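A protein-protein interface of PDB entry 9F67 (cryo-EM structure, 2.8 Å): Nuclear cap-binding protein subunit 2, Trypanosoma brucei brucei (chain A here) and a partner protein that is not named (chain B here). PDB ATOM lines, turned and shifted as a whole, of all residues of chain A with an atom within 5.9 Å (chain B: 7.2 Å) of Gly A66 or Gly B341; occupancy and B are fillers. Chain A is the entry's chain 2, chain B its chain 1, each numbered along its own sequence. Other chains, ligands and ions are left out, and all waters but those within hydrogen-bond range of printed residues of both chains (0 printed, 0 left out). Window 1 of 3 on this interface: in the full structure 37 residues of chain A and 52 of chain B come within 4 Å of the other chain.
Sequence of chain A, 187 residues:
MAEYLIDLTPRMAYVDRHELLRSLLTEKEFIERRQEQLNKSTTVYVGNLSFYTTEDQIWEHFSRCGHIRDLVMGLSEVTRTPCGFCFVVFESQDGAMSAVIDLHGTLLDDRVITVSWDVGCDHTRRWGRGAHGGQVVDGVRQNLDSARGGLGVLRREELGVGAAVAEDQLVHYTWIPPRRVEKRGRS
Among the printed residues, pairs that only touch across the chains: Ser A63 with Gly B341 (3.9 Å), Arg A64 with Arg B342 (3.4 Å), Cys A65 with Arg B342 (3.4 Å), Gly A66 with Gly B341 (3.5 Å), His A67 with Glu B944 (3.2 Å) and Ser A98 with Arg B342 (3.3 Å).
Of the 10 printed residues of chain A, 6 touch a printed residue of chain B. Hydrophobic or aromatic side chains of chain A within 4 Å of the printed part of chain B: His A67. Among the printed residues, no Asp or Glu carboxylate lies within 4 Å of a Lys or Arg side-chain nitrogen of the other chain.
O of Arg A64 lies close to O of Gly B341, 3.2 Å away. The backbone carbonyl oxygen of Arg A64 sits at hydrogen-bond distance from the backbone NH of Cys B343 (2.7 Å). NE of Arg B941 is in hydrogen-bond range of ND1 of His A67. The backbone carbonyl oxygen (O) of Gly B341 sits close to the backbone carbonyl oxygen (O) of Cys A65, at 3.1 Å.
Gly A66 touches just one residue of chain B: Gly B341. Of the printed residues of chain B, Arg A64 touches Gly B341, Arg B342 and Cys B343. Of the printed residues of chain A, Cys B343 touches Arg A64 (2.7 Å). Of the printed residues of chain B, Ser A98 touches Arg B342 (3.3 Å). The nearest residue of chain A that does not touch Gly B341 is His A67 (4.6 Å). The nearest printed residue of chain B that does not touch Arg A64 is Pro B344 (6.0 Å).
NH1 of Arg B941 lies within salt-bridge range of OE2 of Glu B944 (2.4 Å).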
ATOM      1  N   PHE A  62      -0.787  23.767  -3.121  1.00  0.00           N
ATOM      2  CA  PHE A  62       0.080  23.439  -4.290  1.00  0.00           C
ATOM      3  C   PHE A  62      -0.538  22.317  -5.135  1.00  0.00           C
ATOM      4  O   PHE A  62      -0.413  22.381  -6.375  1.00  0.00           O
ATOM      5  CB  PHE A  62       1.530  23.162  -3.869  1.00  0.00           C
ATOM      6  CG  PHE A  62       2.273  24.343  -3.294  1.00  0.00           C
ATOM      7  CD1 PHE A  62       1.851  24.972  -2.133  1.00  0.00           C
ATOM      8  CD2 PHE A  62       3.374  24.865  -3.953  1.00  0.00           C
ATOM      9  CE1 PHE A  62       2.530  26.066  -1.623  1.00  0.00           C
ATOM     10  CE2 PHE A  62       4.050  25.965  -3.449  1.00  0.00           C
ATOM     11  CZ  PHE A  62       3.627  26.563  -2.284  1.00  0.00           C
ATOM     12  N   SER A  63      -1.128  21.302  -4.496  1.00  0.00           N
ATOM     13  CA  SER A  63      -1.670  20.149  -5.264  1.00  0.00           C
ATOM     14  C   SER A  63      -2.712  20.653  -6.266  1.00  0.00           C
ATOM     15  O   SER A  63      -2.800  20.078  -7.368  1.00  0.00           O
ATOM     16  CB  SER A  63      -2.249  19.092  -4.359  1.00  0.00           C
ATOM     17  OG  SER A  63      -3.421  19.567  -3.717  1.00  0.00           O
ATOM     18  N   ARG A  64      -3.455  21.698  -5.893  1.00  0.00           N
ATOM     19  CA  ARG A  64      -4.514  22.245  -6.783  1.00  0.00           C
ATOM     20  C   ARG A  64      -3.913  22.580  -8.150  1.00  0.00           C
ATOM     21  O   ARG A  64      -4.545  22.238  -9.165  1.00  0.00           O
ATOM     22  CB  ARG A  64      -5.140  23.495  -6.159  1.00  0.00           C
ATOM     23  CG  ARG A  64      -5.907  23.231  -4.872  1.00  0.00           C
ATOM     24  CD  ARG A  64      -6.864  22.064  -5.012  1.00  0.00           C
ATOM     25  NE  ARG A  64      -7.874  22.042  -3.965  1.00  0.00           N
ATOM     26  CZ  ARG A  64      -8.928  21.235  -3.958  1.00  0.00           C
ATOM     27  NH1 ARG A  64      -9.096  20.360  -4.933  1.00  0.00           N
ATOM     28  NH2 ARG A  64      -9.816  21.310  -2.980  1.00  0.00           N
ATOM     29  N   CYS A  65      -2.736  23.213  -8.174  1.00  0.00           N
ATOM     30  CA  CYS A  65      -2.145  23.661  -9.465  1.00  0.00           C
ATOM     31  C   CYS A  65      -1.309  22.545 -10.100  1.00  0.00           C
ATOM     32  O   CYS A  65      -1.206  22.533 -11.342  1.00  0.00           O
ATOM     33  CB  CYS A  65      -1.304  24.910  -9.256  1.00  0.00           C
ATOM     34  SG  CYS A  65      -2.332  26.367  -8.943  1.00  0.00           S
ATOM     35  N   GLY A  66      -0.722  21.656  -9.294  1.00  0.00           N
ATOM     36  CA  GLY A  66      -0.009  20.509  -9.895  1.00  0.00           C
ATOM     37  C   GLY A  66       0.262  19.380  -8.916  1.00  0.00           C
ATOM     38  O   GLY A  66       0.355  19.665  -7.708  1.00  0.00           O
ATOM     39  N   HIS A  67       0.447  18.151  -9.415  1.00  0.00           N
ATOM     40  CA  HIS A  67       0.833  17.025  -8.521  1.00  0.00           C
ATOM     41  C   HIS A  67       2.238  17.308  -7.986  1.00  0.00           C
ATOM     42  O   HIS A  67       3.111  17.725  -8.777  1.00  0.00           O
ATOM     43  CB  HIS A  67       0.745  15.688  -9.268  1.00  0.00           C
ATOM     44  CG  HIS A  67       1.205  14.479  -8.513  1.00  0.00           C
ATOM     45  ND1 HIS A  67       0.355  13.434  -8.223  1.00  0.00           N
ATOM     46  CD2 HIS A  67       2.390  14.143  -7.982  1.00  0.00           C
ATOM     47  CE1 HIS A  67       1.016  12.503  -7.550  1.00  0.00           C
ATOM     48  NE2 HIS A  67       2.255  12.915  -7.391  1.00  0.00           N
ATOM     49  N   ILE A  68       2.466  17.034  -6.699  1.00  0.00           N
ATOM     50  CA  ILE A  68       3.789  17.354  -6.093  1.00  0.00           C
ATOM     51  C   ILE A  68       4.612  16.065  -6.023  1.00  0.00           C
ATOM     52  O   ILE A  68       4.229  15.162  -5.253  1.00  0.00           O
ATOM     53  CB  ILE A  68       3.573  17.973  -4.698  1.00  0.00           C
ATOM     54  CG1 ILE A  68       2.632  19.178  -4.756  1.00  0.00           C
ATOM     55  CG2 ILE A  68       4.894  18.324  -4.039  1.00  0.00           C
ATOM     56  CD1 ILE A  68       2.441  19.869  -3.431  1.00  0.00           C
ATOM     57  N   PHE A  90       7.588  19.379  -8.373  1.00  0.00           N
ATOM     58  CA  PHE A  90       6.420  18.918  -9.166  1.00  0.00           C
ATOM     59  C   PHE A  90       6.878  17.934 -10.242  1.00  0.00           C
ATOM     60  O   PHE A  90       7.988  18.090 -10.771  1.00  0.00           O
ATOM     61  CB  PHE A  90       5.724  20.117  -9.810  1.00  0.00           C
ATOM     62  CG  PHE A  90       5.026  21.046  -8.853  1.00  0.00           C
ATOM     63  CD1 PHE A  90       3.966  20.604  -8.078  1.00  0.00           C
ATOM     64  CD2 PHE A  90       5.459  22.349  -8.686  1.00  0.00           C
ATOM     65  CE1 PHE A  90       3.321  21.460  -7.200  1.00  0.00           C
ATOM     66  CE2 PHE A  90       4.822  23.201  -7.799  1.00  0.00           C
ATOM     67  CZ  PHE A  90       3.752  22.757  -7.061  1.00  0.00           C
ATOM     68  N   GLY A  95       3.302  22.348 -13.971  1.00  0.00           N
ATOM     69  CA  GLY A  95       2.733  22.469 -12.615  1.00  0.00           C
ATOM     70  C   GLY A  95       3.522  23.475 -11.796  1.00  0.00           C
ATOM     71  O   GLY A  95       2.889  24.245 -11.051  1.00  0.00           O
ATOM     72  N   SER A  98       2.493  26.706 -13.017  1.00  0.00           N
ATOM     73  CA  SER A  98       1.154  27.013 -12.461  1.00  0.00           C
ATOM     74  C   SER A  98       1.324  27.518 -11.031  1.00  0.00           C
ATOM     75  O   SER A  98       0.707  28.543 -10.686  1.00  0.00           O
ATOM     76  CB  SER A  98       0.307  25.776 -12.452  1.00  0.00           C
ATOM     77  OG  SER A  98       0.220  25.202 -13.746  1.00  0.00           O
ATOM     78  N   ASP B 338      -7.460  18.573 -20.354  1.00  0.00           N
ATOM     79  CA  ASP B 338      -6.289  19.276 -20.853  1.00  0.00           C
ATOM     80  C   ASP B 338      -4.968  18.677 -20.403  1.00  0.00           C
ATOM     81  O   ASP B 338      -3.925  19.090 -20.920  1.00  0.00           O
ATOM     82  CB  ASP B 338      -6.339  20.751 -20.440  1.00  0.00           C
ATOM     83  CG  ASP B 338      -6.664  20.929 -18.985  1.00  0.00           C
ATOM     84  OD1 ASP B 338      -7.628  20.295 -18.511  1.00  0.00           O
ATOM     85  OD2 ASP B 338      -5.976  21.719 -18.315  1.00  0.00           O
ATOM     86  N   GLY B 339      -4.975  17.727 -19.474  1.00  0.00           N
ATOM     87  CA  GLY B 339      -3.765  17.050 -19.066  1.00  0.00           C
ATOM     88  C   GLY B 339      -2.727  17.929 -18.406  1.00  0.00           C
ATOM     89  O   GLY B 339      -1.549  17.862 -18.765  1.00  0.00           O
ATOM     90  N   THR B 340      -3.138  18.767 -17.452  1.00  0.00           N
ATOM     91  CA  THR B 340      -2.195  19.623 -16.747  1.00  0.00           C
ATOM     92  C   THR B 340      -2.257  19.521 -15.231  1.00  0.00           C
ATOM     93  O   THR B 340      -1.318  19.979 -14.571  1.00  0.00           O
ATOM     94  CB  THR B 340      -2.391  21.094 -17.143  1.00  0.00           C
ATOM     95  OG1 THR B 340      -1.230  21.844 -16.768  1.00  0.00           O
ATOM     96  CG2 THR B 340      -3.586  21.679 -16.430  1.00  0.00           C
ATOM     97  N   GLY B 341      -3.311  18.951 -14.657  1.00  0.00           N
ATOM     98  CA  GLY B 341      -3.355  18.810 -13.217  1.00  0.00           C
ATOM     99  C   GLY B 341      -3.556  20.100 -12.462  1.00  0.00           C
ATOM    100  O   GLY B 341      -3.254  20.166 -11.268  1.00  0.00           O
ATOM    101  N   ARG B 342      -4.058  21.131 -13.129  1.00  0.00           N
ATOM    102  CA  ARG B 342      -4.364  22.413 -12.517  1.00  0.00           C
ATOM    103  C   ARG B 342      -5.869  22.522 -12.343  1.00  0.00           C
ATOM    104  O   ARG B 342      -6.623  22.297 -13.296  1.00  0.00           O
ATOM    105  CB  ARG B 342      -3.836  23.560 -13.376  1.00  0.00           C
ATOM    106  CG  ARG B 342      -3.832  24.900 -12.691  1.00  0.00           C
ATOM    107  CD  ARG B 342      -3.015  25.899 -13.477  1.00  0.00           C
ATOM    108  NE  ARG B 342      -3.668  27.197 -13.578  1.00  0.00           N
ATOM    109  CZ  ARG B 342      -4.482  27.547 -14.564  1.00  0.00           C
ATOM    110  NH1 ARG B 342      -4.774  26.714 -15.548  1.00  0.00           N
ATOM    111  NH2 ARG B 342      -5.016  28.765 -14.562  1.00  0.00           N
ATOM    112  N   CYS B 343      -6.302  22.857 -11.135  1.00  0.00           N
ATOM    113  CA  CYS B 343      -7.725  22.910 -10.833  1.00  0.00           C
ATOM    114  C   CYS B 343      -8.326  24.204 -11.361  1.00  0.00           C
ATOM    115  O   CYS B 343      -7.908  25.286 -10.934  1.00  0.00           O
ATOM    116  CB  CYS B 343      -7.959  22.807  -9.336  1.00  0.00           C
ATOM    117  SG  CYS B 343      -9.585  22.182  -8.891  1.00  0.00           S
ATOM    118  N   PRO B 344      -9.294  24.144 -12.274  1.00  0.00           N
ATOM    119  CA  PRO B 344      -9.918  25.383 -12.756  1.00  0.00           C
ATOM    120  C   PRO B 344     -10.632  26.166 -11.673  1.00  0.00           C
ATOM    121  O   PRO B 344     -10.680  27.400 -11.745  1.00  0.00           O
ATOM    122  CB  PRO B 344     -10.891  24.885 -13.831  1.00  0.00           C
ATOM    123  CG  PRO B 344     -11.088  23.445 -13.537  1.00  0.00           C
ATOM    124  CD  PRO B 344      -9.810  22.959 -12.969  1.00  0.00           C
ATOM    125  N   SER B 940      -8.240  12.165 -13.880  1.00  0.00           N
ATOM    126  CA  SER B 940      -7.470  13.389 -14.084  1.00  0.00           C
ATOM    127  C   SER B 940      -5.980  13.129 -13.900  1.00  0.00           C
ATOM    128  O   SER B 940      -5.151  13.578 -14.705  1.00  0.00           O
ATOM    129  CB  SER B 940      -7.953  14.477 -13.128  1.00  0.00           C
ATOM    130  OG  SER B 940      -6.929  15.425 -12.880  1.00  0.00           O
ATOM    131  N   ARG B 941      -5.622  12.383 -12.853  1.00  0.00           N
ATOM    132  CA  ARG B 941      -4.225  12.059 -12.600  1.00  0.00           C
ATOM    133  C   ARG B 941      -3.649  11.180 -13.698  1.00  0.00           C
ATOM    134  O   ARG B 941      -2.501  11.372 -14.112  1.00  0.00           O
ATOM    135  CB  ARG B 941      -4.091  11.379 -11.242  1.00  0.00           C
ATOM    136  CG  ARG B 941      -2.732  10.787 -10.978  1.00  0.00           C
ATOM    137  CD  ARG B 941      -1.749  11.847 -10.553  1.00  0.00           C
ATOM    138  NE  ARG B 941      -0.413  11.299 -10.367  1.00  0.00           N
ATOM    139  CZ  ARG B 941       0.652  11.679 -11.057  1.00  0.00           C
ATOM    140  NH1 ARG B 941       0.574  12.612 -11.989  1.00  0.00           N
ATOM    141  NH2 ARG B 941       1.826  11.108 -10.803  1.00  0.00           N
ATOM    142  N   LEU B 943      -4.517  11.106 -16.853  1.00  0.00           N
ATOM    143  CA  LEU B 943      -4.285  11.942 -18.027  1.00  0.00           C
ATOM    144  C   LEU B 943      -3.074  12.847 -17.838  1.00  0.00           C
ATOM    145  O   LEU B 943      -2.269  13.023 -18.764  1.00  0.00           O
ATOM    146  CB  LEU B 943      -5.529  12.769 -18.338  1.00  0.00           C
ATOM    147  CG  LEU B 943      -6.597  12.110 -19.206  1.00  0.00           C
ATOM    148  CD1 LEU B 943      -7.490  13.167 -19.812  1.00  0.00           C
ATOM    149  CD2 LEU B 943      -5.961  11.270 -20.287  1.00  0.00           C
ATOM    150  N   GLU B 944      -2.921  13.431 -16.650  1.00  0.00           N
ATOM    151  CA  GLU B 944      -1.783  14.313 -16.419  1.00  0.00           C
ATOM    152  C   GLU B 944      -0.466  13.549 -16.491  1.00  0.00           C
ATOM    153  O   GLU B 944       0.512  14.025 -17.086  1.00  0.00           O
ATOM    154  CB  GLU B 944      -1.928  15.014 -15.073  1.00  0.00           C
ATOM    155  CG  GLU B 944      -0.616  15.395 -14.442  1.00  0.00           C
ATOM    156  CD  GLU B 944      -0.676  15.380 -12.936  1.00  0.00           C
ATOM    157  OE1 GLU B 944      -1.727  15.753 -12.376  1.00  0.00           O
ATOM    158  OE2 GLU B 944       0.329  14.985 -12.314  1.00  0.00           O
ATOM    159  N   SER B 947       0.395  12.922 -20.036  1.00  0.00           N
ATOM    160  CA  SER B 947       0.972  14.110 -20.656  1.00  0.00           C
ATOM    161  C   SER B 947       2.441  14.270 -20.285  1.00  0.00           C
ATOM    162  O   SER B 947       3.275  14.580 -21.145  1.00  0.00           O
ATOM    163  CB  SER B 947       0.182  15.352 -20.252  1.00  0.00           C
ATOM    164  OG  SER B 947       0.278  15.579 -18.858  1.00  0.00           O
